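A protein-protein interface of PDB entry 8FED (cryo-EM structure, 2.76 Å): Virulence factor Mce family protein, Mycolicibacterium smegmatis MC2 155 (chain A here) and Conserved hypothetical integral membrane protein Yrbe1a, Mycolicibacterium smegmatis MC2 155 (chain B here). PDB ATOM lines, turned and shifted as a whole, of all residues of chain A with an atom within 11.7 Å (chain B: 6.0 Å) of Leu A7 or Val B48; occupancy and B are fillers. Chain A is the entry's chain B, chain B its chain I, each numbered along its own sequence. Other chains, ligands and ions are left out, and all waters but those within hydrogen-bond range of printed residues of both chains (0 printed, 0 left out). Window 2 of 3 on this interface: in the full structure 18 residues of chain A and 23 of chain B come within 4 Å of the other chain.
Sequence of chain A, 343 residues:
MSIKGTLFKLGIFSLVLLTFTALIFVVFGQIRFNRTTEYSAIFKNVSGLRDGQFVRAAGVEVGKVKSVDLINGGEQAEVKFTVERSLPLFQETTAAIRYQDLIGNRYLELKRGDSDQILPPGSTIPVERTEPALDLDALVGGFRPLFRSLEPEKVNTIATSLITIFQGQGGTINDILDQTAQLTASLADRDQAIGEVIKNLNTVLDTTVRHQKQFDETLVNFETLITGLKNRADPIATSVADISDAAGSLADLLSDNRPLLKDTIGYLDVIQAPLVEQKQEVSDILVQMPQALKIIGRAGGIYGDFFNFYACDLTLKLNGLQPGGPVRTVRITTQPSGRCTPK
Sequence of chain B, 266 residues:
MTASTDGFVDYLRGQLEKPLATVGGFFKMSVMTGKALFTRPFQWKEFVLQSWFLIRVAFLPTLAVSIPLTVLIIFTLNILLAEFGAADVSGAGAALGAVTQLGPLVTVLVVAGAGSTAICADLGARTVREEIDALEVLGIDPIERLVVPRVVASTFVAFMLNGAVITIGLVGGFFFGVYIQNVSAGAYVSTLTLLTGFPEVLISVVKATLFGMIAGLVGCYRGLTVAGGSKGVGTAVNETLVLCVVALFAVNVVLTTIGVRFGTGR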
ATOM      1  N   ILE A   3      -3.901  10.462  -9.238  1.00  0.00           N
ATOM      2  CA  ILE A   3      -4.064   9.643  -8.045  1.00  0.00           C
ATOM      3  C   ILE A   3      -5.324   8.793  -8.191  1.00  0.00           C
ATOM      4  O   ILE A   3      -5.475   7.769  -7.528  1.00  0.00           O
ATOM      5  CB  ILE A   3      -4.107  10.522  -6.771  1.00  0.00           C
ATOM      6  CG1 ILE A   3      -4.067   9.661  -5.505  1.00  0.00           C
ATOM      7  CG2 ILE A   3      -5.333  11.424  -6.777  1.00  0.00           C
ATOM      8  CD1 ILE A   3      -4.155  10.453  -4.222  1.00  0.00           C
ATOM      9  N   LYS A   4      -6.217   9.218  -9.088  1.00  0.00           N
ATOM     10  CA  LYS A   4      -7.475   8.504  -9.292  1.00  0.00           C
ATOM     11  C   LYS A   4      -7.228   7.098  -9.827  1.00  0.00           C
ATOM     12  O   LYS A   4      -7.763   6.114  -9.299  1.00  0.00           O
ATOM     13  CB  LYS A   4      -8.371   9.299 -10.242  1.00  0.00           C
ATOM     14  CG  LYS A   4      -9.857   9.023 -10.091  1.00  0.00           C
ATOM     15  CD  LYS A   4     -10.360   9.500  -8.739  1.00  0.00           C
ATOM     16  CE  LYS A   4     -11.875   9.628  -8.720  1.00  0.00           C
ATOM     17  NZ  LYS A   4     -12.556   8.358  -9.091  1.00  0.00           N
ATOM     18  N   GLY A   5      -6.413   6.986 -10.879  1.00  0.00           N
ATOM     19  CA  GLY A   5      -6.079   5.674 -11.409  1.00  0.00           C
ATOM     20  C   GLY A   5      -5.289   4.833 -10.426  1.00  0.00           C
ATOM     21  O   GLY A   5      -5.520   3.628 -10.298  1.00  0.00           O
ATOM     22  N   THR A   6      -4.340   5.457  -9.722  1.00  0.00           N
ATOM     23  CA  THR A   6      -3.601   4.750  -8.682  1.00  0.00           C
ATOM     24  C   THR A   6      -4.537   4.274  -7.580  1.00  0.00           C
ATOM     25  O   THR A   6      -4.395   3.152  -7.076  1.00  0.00           O
ATOM     26  CB  THR A   6      -2.508   5.655  -8.112  1.00  0.00           C
ATOM     27  OG1 THR A   6      -1.556   5.963  -9.137  1.00  0.00           O
ATOM     28  CG2 THR A   6      -1.791   4.978  -6.954  1.00  0.00           C
ATOM     29  N   LEU A   7      -5.506   5.111  -7.198  1.00  0.00           N
ATOM     30  CA  LEU A   7      -6.475   4.709  -6.182  1.00  0.00           C
ATOM     31  C   LEU A   7      -7.299   3.519  -6.652  1.00  0.00           C
ATOM     32  O   LEU A   7      -7.548   2.588  -5.880  1.00  0.00           O
ATOM     33  CB  LEU A   7      -7.386   5.882  -5.822  1.00  0.00           C
ATOM     34  CG  LEU A   7      -8.368   5.636  -4.676  1.00  0.00           C
ATOM     35  CD1 LEU A   7      -7.625   5.235  -3.416  1.00  0.00           C
ATOM     36  CD2 LEU A   7      -9.216   6.871  -4.430  1.00  0.00           C
ATOM     37  N   PHE A   8      -7.733   3.533  -7.916  1.00  0.00           N
ATOM     38  CA  PHE A   8      -8.504   2.409  -8.442  1.00  0.00           C
ATOM     39  C   PHE A   8      -7.677   1.128  -8.464  1.00  0.00           C
ATOM     40  O   PHE A   8      -8.173   0.056  -8.094  1.00  0.00           O
ATOM     41  CB  PHE A   8      -9.024   2.736  -9.841  1.00  0.00           C
ATOM     42  CG  PHE A   8     -10.245   3.611  -9.846  1.00  0.00           C
ATOM     43  CD1 PHE A   8     -10.971   3.818  -8.684  1.00  0.00           C
ATOM     44  CD2 PHE A   8     -10.673   4.219 -11.015  1.00  0.00           C
ATOM     45  CE1 PHE A   8     -12.096   4.620  -8.687  1.00  0.00           C
ATOM     46  CE2 PHE A   8     -11.798   5.022 -11.024  1.00  0.00           C
ATOM     47  CZ  PHE A   8     -12.511   5.221  -9.859  1.00  0.00           C
ATOM     48  N   LYS A   9      -6.418   1.217  -8.906  1.00  0.00           N
ATOM     49  CA  LYS A   9      -5.562   0.033  -8.942  1.00  0.00           C
ATOM     50  C   LYS A   9      -5.325  -0.520  -7.543  1.00  0.00           C
ATOM     51  O   LYS A   9      -5.399  -1.738  -7.326  1.00  0.00           O
ATOM     52  CB  LYS A   9      -4.230   0.359  -9.618  1.00  0.00           C
ATOM     53  CG  LYS A   9      -4.349   0.761 -11.077  1.00  0.00           C
ATOM     54  CD  LYS A   9      -3.019   1.263 -11.613  1.00  0.00           C
ATOM     55  CE  LYS A   9      -3.182   1.904 -12.980  1.00  0.00           C
ATOM     56  NZ  LYS A   9      -1.908   2.498 -13.468  1.00  0.00           N
ATOM     57  N   LEU A  10      -5.034   0.362  -6.582  1.00  0.00           N
ATOM     58  CA  LEU A  10      -4.827  -0.080  -5.208  1.00  0.00           C
ATOM     59  C   LEU A  10      -6.091  -0.706  -4.640  1.00  0.00           C
ATOM     60  O   LEU A  10      -6.026  -1.725  -3.947  1.00  0.00           O
ATOM     61  CB  LEU A  10      -4.372   1.090  -4.336  1.00  0.00           C
ATOM     62  CG  LEU A  10      -4.242   0.770  -2.846  1.00  0.00           C
ATOM     63  CD1 LEU A  10      -3.175  -0.283  -2.616  1.00  0.00           C
ATOM     64  CD2 LEU A  10      -3.947   2.017  -2.037  1.00  0.00           C
ATOM     65  N   GLY A  11      -7.253  -0.115  -4.930  1.00  0.00           N
ATOM     66  CA  GLY A  11      -8.502  -0.683  -4.451  1.00  0.00           C
ATOM     67  C   GLY A  11      -8.775  -2.062  -5.017  1.00  0.00           C
ATOM     68  O   GLY A  11      -9.186  -2.968  -4.292  1.00  0.00           O
ATOM     69  N   ILE A  12      -8.536  -2.243  -6.318  1.00  0.00           N
ATOM     70  CA  ILE A  12      -8.771  -3.542  -6.948  1.00  0.00           C
ATOM     71  C   ILE A  12      -7.827  -4.595  -6.376  1.00  0.00           C
ATOM     72  O   ILE A  12      -8.248  -5.706  -6.022  1.00  0.00           O
ATOM     73  CB  ILE A  12      -8.635  -3.428  -8.477  1.00  0.00           C
ATOM     74  CG1 ILE A  12      -9.800  -2.626  -9.056  1.00  0.00           C
ATOM     75  CG2 ILE A  12      -8.562  -4.807  -9.116  1.00  0.00           C
ATOM     76  CD1 ILE A  12      -9.783  -2.526 -10.564  1.00  0.00           C
ATOM     77  N   PHE A  13      -6.536  -4.262  -6.275  1.00  0.00           N
ATOM     78  CA  PHE A  13      -5.573  -5.219  -5.738  1.00  0.00           C
ATOM     79  C   PHE A  13      -5.874  -5.553  -4.283  1.00  0.00           C
ATOM     80  O   PHE A  13      -5.783  -6.718  -3.874  1.00  0.00           O
ATOM     81  CB  PHE A  13      -4.153  -4.673  -5.880  1.00  0.00           C
ATOM     82  CG  PHE A  13      -3.452  -5.134  -7.122  1.00  0.00           C
ATOM     83  CD1 PHE A  13      -3.743  -4.565  -8.349  1.00  0.00           C
ATOM     84  CD2 PHE A  13      -2.499  -6.137  -7.061  1.00  0.00           C
ATOM     85  CE1 PHE A  13      -3.098  -4.987  -9.495  1.00  0.00           C
ATOM     86  CE2 PHE A  13      -1.850  -6.564  -8.202  1.00  0.00           C
ATOM     87  CZ  PHE A  13      -2.150  -5.989  -9.422  1.00  0.00           C
ATOM     88  N   SER A  14      -6.232  -4.542  -3.486  1.00  0.00           N
ATOM     89  CA  SER A  14      -6.585  -4.781  -2.095  1.00  0.00           C
ATOM     90  C   SER A  14      -7.819  -5.660  -1.985  1.00  0.00           C
ATOM     91  O   SER A  14      -7.870  -6.559  -1.144  1.00  0.00           O
ATOM     92  CB  SER A  14      -6.806  -3.453  -1.375  1.00  0.00           C
ATOM     93  OG  SER A  14      -5.653  -2.635  -1.458  1.00  0.00           O
ATOM     94  N   LEU A  15      -8.822  -5.420  -2.834  1.00  0.00           N
ATOM     95  CA  LEU A  15     -10.020  -6.250  -2.818  1.00  0.00           C
ATOM     96  C   LEU A  15      -9.687  -7.702  -3.138  1.00  0.00           C
ATOM     97  O   LEU A  15     -10.151  -8.616  -2.448  1.00  0.00           O
ATOM     98  CB  LEU A  15     -11.047  -5.701  -3.807  1.00  0.00           C
ATOM     99  CG  LEU A  15     -12.447  -6.310  -3.763  1.00  0.00           C
ATOM    100  CD1 LEU A  15     -13.109  -6.030  -2.424  1.00  0.00           C
ATOM    101  CD2 LEU A  15     -13.294  -5.775  -4.905  1.00  0.00           C
ATOM    102  N   VAL A  16      -8.857  -7.929  -4.160  1.00  0.00           N
ATOM    103  CA  VAL A  16      -8.513  -9.297  -4.550  1.00  0.00           C
ATOM    104  C   VAL A  16      -7.736  -9.999  -3.438  1.00  0.00           C
ATOM    105  O   VAL A  16      -8.018 -11.153  -3.087  1.00  0.00           O
ATOM    106  CB  VAL A  16      -7.732  -9.296  -5.875  1.00  0.00           C
ATOM    107  CG1 VAL A  16      -7.228 -10.691  -6.196  1.00  0.00           C
ATOM    108  CG2 VAL A  16      -8.608  -8.779  -7.000  1.00  0.00           C
ATOM    109  N   GLN B  43      -2.669  10.952   6.499  1.00  0.00           N
ATOM    110  CA  GLN B  43      -2.373  11.328   5.117  1.00  0.00           C
ATOM    111  C   GLN B  43      -2.834  10.195   4.207  1.00  0.00           C
ATOM    112  O   GLN B  43      -2.132   9.198   4.037  1.00  0.00           O
ATOM    113  CB  GLN B  43      -0.884  11.607   4.945  1.00  0.00           C
ATOM    114  CG  GLN B  43      -0.366  12.778   5.758  1.00  0.00           C
ATOM    115  CD  GLN B  43      -0.672  14.113   5.114  1.00  0.00           C
ATOM    116  OE1 GLN B  43      -0.835  14.204   3.898  1.00  0.00           O
ATOM    117  NE2 GLN B  43      -0.754  15.157   5.929  1.00  0.00           N
ATOM    118  N   TRP B  44      -4.020  10.353   3.614  1.00  0.00           N
ATOM    119  CA  TRP B  44      -4.572   9.288   2.782  1.00  0.00           C
ATOM    120  C   TRP B  44      -3.869   9.205   1.432  1.00  0.00           C
ATOM    121  O   TRP B  44      -3.623   8.103   0.925  1.00  0.00           O
ATOM    122  CB  TRP B  44      -6.074   9.493   2.593  1.00  0.00           C
ATOM    123  CG  TRP B  44      -6.858   9.271   3.847  1.00  0.00           C
ATOM    124  CD1 TRP B  44      -7.383  10.226   4.666  1.00  0.00           C
ATOM    125  CD2 TRP B  44      -7.192   8.009   4.436  1.00  0.00           C
ATOM    126  NE1 TRP B  44      -8.031   9.637   5.724  1.00  0.00           N
ATOM    127  CE2 TRP B  44      -7.927   8.276   5.607  1.00  0.00           C
ATOM    128  CE3 TRP B  44      -6.945   6.679   4.084  1.00  0.00           C
ATOM    129  CZ2 TRP B  44      -8.416   7.264   6.428  1.00  0.00           C
ATOM    130  CZ3 TRP B  44      -7.431   5.675   4.902  1.00  0.00           C
ATOM    131  CH2 TRP B  44      -8.158   5.973   6.059  1.00  0.00           C
ATOM    132  N   LYS B  45      -3.549  10.352   0.830  1.00  0.00           N
ATOM    133  CA  LYS B  45      -2.917  10.352  -0.487  1.00  0.00           C
ATOM    134  C   LYS B  45      -1.544   9.693  -0.438  1.00  0.00           C
ATOM    135  O   LYS B  45      -1.214   8.847  -1.280  1.00  0.00           O
ATOM    136  CB  LYS B  45      -2.809  11.783  -1.012  1.00  0.00           C
ATOM    137  CG  LYS B  45      -4.081  12.595  -0.844  1.00  0.00           C
ATOM    138  CD  LYS B  45      -3.894  14.026  -1.314  1.00  0.00           C
ATOM    139  CE  LYS B  45      -5.126  14.864  -1.019  1.00  0.00           C
ATOM    140  NZ  LYS B  45      -6.352  14.275  -1.624  1.00  0.00           N
ATOM    141  N   GLU B  46      -0.730  10.070   0.551  1.00  0.00           N
ATOM    142  CA  GLU B  46       0.602   9.487   0.677  1.00  0.00           C
ATOM    143  C   GLU B  46       0.519   8.002   1.001  1.00  0.00           C
ATOM    144  O   GLU B  46       1.323   7.208   0.501  1.00  0.00           O
ATOM    145  CB  GLU B  46       1.406  10.234   1.739  1.00  0.00           C
ATOM    146  CG  GLU B  46       2.909  10.004   1.653  1.00  0.00           C
ATOM    147  CD  GLU B  46       3.518  10.547   0.371  1.00  0.00           C
ATOM    148  OE1 GLU B  46       2.959  11.506  -0.202  1.00  0.00           O
ATOM    149  OE2 GLU B  46       4.559  10.013  -0.065  1.00  0.00           O
ATOM    150  N   PHE B  47      -0.443   7.611   1.841  1.00  0.00           N
ATOM    151  CA  PHE B  47      -0.637   6.197   2.147  1.00  0.00           C
ATOM    152  C   PHE B  47      -0.983   5.405   0.894  1.00  0.00           C
ATOM    153  O   PHE B  47      -0.440   4.319   0.673  1.00  0.00           O
ATOM    154  CB  PHE B  47      -1.725   6.038   3.208  1.00  0.00           C
ATOM    155  CG  PHE B  47      -2.394   4.692   3.206  1.00  0.00           C
ATOM    156  CD1 PHE B  47      -1.808   3.611   3.839  1.00  0.00           C
ATOM    157  CD2 PHE B  47      -3.624   4.514   2.591  1.00  0.00           C
ATOM    158  CE1 PHE B  47      -2.425   2.374   3.841  1.00  0.00           C
ATOM    159  CE2 PHE B  47      -4.242   3.280   2.590  1.00  0.00           C
ATOM    160  CZ  PHE B  47      -3.643   2.210   3.217  1.00  0.00           C
ATOM    161  N   VAL B  48      -1.886   5.931   0.063  1.00  0.00           N
ATOM    162  CA  VAL B  48      -2.250   5.243  -1.174  1.00  0.00           C
ATOM    163  C   VAL B  48      -1.043   5.127  -2.095  1.00  0.00           C
ATOM    164  O   VAL B  48      -0.780   4.061  -2.671  1.00  0.00           O
ATOM    165  CB  VAL B  48      -3.422   5.967  -1.864  1.00  0.00           C
ATOM    166  CG1 VAL B  48      -3.605   5.462  -3.285  1.00  0.00           C
ATOM    167  CG2 VAL B  48      -4.701   5.770  -1.070  1.00  0.00           C
ATOM    168  N   LEU B  49      -0.286   6.219  -2.241  1.00  0.00           N
ATOM    169  CA  LEU B  49       0.875   6.200  -3.126  1.00  0.00           C
ATOM    170  C   LEU B  49       1.915   5.191  -2.656  1.00  0.00           C
ATOM    171  O   LEU B  49       2.452   4.421  -3.462  1.00  0.00           O
ATOM    172  CB  LEU B  49       1.485   7.596  -3.224  1.00  0.00           C
ATOM    173  CG  LEU B  49       0.641   8.650  -3.942  1.00  0.00           C
ATOM    174  CD1 LEU B  49       1.349   9.992  -3.938  1.00  0.00           C
ATOM    175  CD2 LEU B  49       0.334   8.209  -5.361  1.00  0.00           C
ATOM    176  N   GLN B  50       2.199   5.161  -1.351  1.00  0.00           N
ATOM    177  CA  GLN B  50       3.208   4.239  -0.839  1.00  0.00           C
ATOM    178  C   GLN B  50       2.727   2.795  -0.893  1.00  0.00           C
ATOM    179  O   GLN B  50       3.521   1.886  -1.155  1.00  0.00           O
ATOM    180  CB  GLN B  50       3.609   4.626   0.583  1.00  0.00           C
ATOM    181  CG  GLN B  50       4.257   5.993   0.685  1.00  0.00           C
ATOM    182  CD  GLN B  50       5.371   6.188  -0.323  1.00  0.00           C
ATOM    183  OE1 GLN B  50       6.259   5.346  -0.456  1.00  0.00           O
ATOM    184  NE2 GLN B  50       5.329   7.302  -1.044  1.00  0.00           N
ATOM    185  N   SER B  51       1.433   2.560  -0.651  1.00  0.00           N
ATOM    186  CA  SER B  51       0.891   1.212  -0.777  1.00  0.00           C
ATOM    187  C   SER B  51       1.037   0.702  -2.202  1.00  0.00           C
ATOM    188  O   SER B  51       1.486  -0.429  -2.429  1.00  0.00           O
ATOM    189  CB  SER B  51      -0.576   1.191  -0.350  1.00  0.00           C
ATOM    190  OG  SER B  51      -0.730   1.603   0.994  1.00  0.00           O
ATOM    191  N   TRP B  52       0.677   1.534  -3.183  1.00  0.00           N
ATOM    192  CA  TRP B  52       0.799   1.105  -4.571  1.00  0.00           C
ATOM    193  C   TRP B  52       2.257   0.925  -4.967  1.00  0.00           C
ATOM    194  O   TRP B  52       2.585   0.020  -5.742  1.00  0.00           O
ATOM    195  CB  TRP B  52       0.106   2.093  -5.506  1.00  0.00           C
ATOM    196  CG  TRP B  52       0.266   1.729  -6.951  1.00  0.00           C
ATOM    197  CD1 TRP B  52       0.849   2.485  -7.922  1.00  0.00           C
ATOM    198  CD2 TRP B  52      -0.143   0.508  -7.584  1.00  0.00           C
ATOM    199  NE1 TRP B  52       0.820   1.819  -9.122  1.00  0.00           N
ATOM    200  CE2 TRP B  52       0.217   0.603  -8.942  1.00  0.00           C
ATOM    201  CE3 TRP B  52      -0.785  -0.651  -7.136  1.00  0.00           C
ATOM    202  CZ2 TRP B  52      -0.042  -0.416  -9.854  1.00  0.00           C
ATOM    203  CZ3 TRP B  52      -1.039  -1.661  -8.044  1.00  0.00           C
ATOM    204  CH2 TRP B  52      -0.668  -1.537  -9.387  1.00  0.00           C
ATOM    205  N   PHE B  53       3.147   1.776  -4.451  1.00  0.00           N
ATOM    206  CA  PHE B  53       4.568   1.630  -4.750  1.00  0.00           C
ATOM    207  C   PHE B  53       5.112   0.315  -4.207  1.00  0.00           C
ATOM    208  O   PHE B  53       5.823  -0.414  -4.911  1.00  0.00           O
ATOM    209  CB  PHE B  53       5.345   2.816  -4.180  1.00  0.00           C
ATOM    210  CG  PHE B  53       6.835   2.651  -4.245  1.00  0.00           C
ATOM    211  CD1 PHE B  53       7.484   2.582  -5.466  1.00  0.00           C
ATOM    212  CD2 PHE B  53       7.587   2.573  -3.086  1.00  0.00           C
ATOM    213  CE1 PHE B  53       8.854   2.431  -5.529  1.00  0.00           C
ATOM    214  CE2 PHE B  53       8.956   2.425  -3.143  1.00  0.00           C
ATOM    215  CZ  PHE B  53       9.591   2.354  -4.365  1.00  0.00           C
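The backbone carbonyl oxygen (O) of Leu A10 is in hydrogen-bond range of the side-chain hydroxyl (OG) of Ser A14. The side-chain hydroxyl of Ser B51 sits at hydrogen-bond distance from the backbone carbonyl oxygen of Phe B47 (2.8 Å).
Among the printed residues, pairs that only touch across the chains: Ile A3 with Lys B45 (3.7 Å), Thr A6 with Trp B52 (3.7 Å), Leu A7 with Val B48 (3.8 Å), Lys A9 with Trp B52 (3.8 Å), Leu A10 with Val B48 (3.7 Å), Leu A10 with Ser B51 (3.7 Å) and Phe A13 with Trp B52 (3.98 Å).
Of the printed residues of chain B, Leu A7 touches Val B48. No residue of chain A comes within 4 Å of Glu B46. No residue of chain A comes within 4 Å of Phe B47. Leu B49 touches none of the printed residues of chain A. No residue of chain A comes within 4 Å of Gln B50. Printed residues of chain A within 4 Å of Lys B45: Ile A3. Printed residues of chain B within 4 Å of Leu A10: Val B48 (3.7 Å) and Ser B51 (3.7 Å). Printed residues of chain A within 4 Å of Trp B52: Thr A6 (3.7 Å), Lys A9 (3.8 Å) and Phe A13 (3.98 Å). Printed residues of chain B within 4 Å of Thr A6: Trp B52 (3.7 Å). Of the printed residues of chain B, Ile A3 touches Lys B45.
Hydrophobic or aromatic side chains of chain B within 4 Å of the printed part of chain A: Val B48 and Trp B52. Of the 14 printed residues of chain A, 6 touch a printed residue of chain B. Hydrophobic or aromatic side chains of chain A within 4 Å of the printed part of chain B: Ile A3, Leu A7, Leu A10 and Phe A13.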
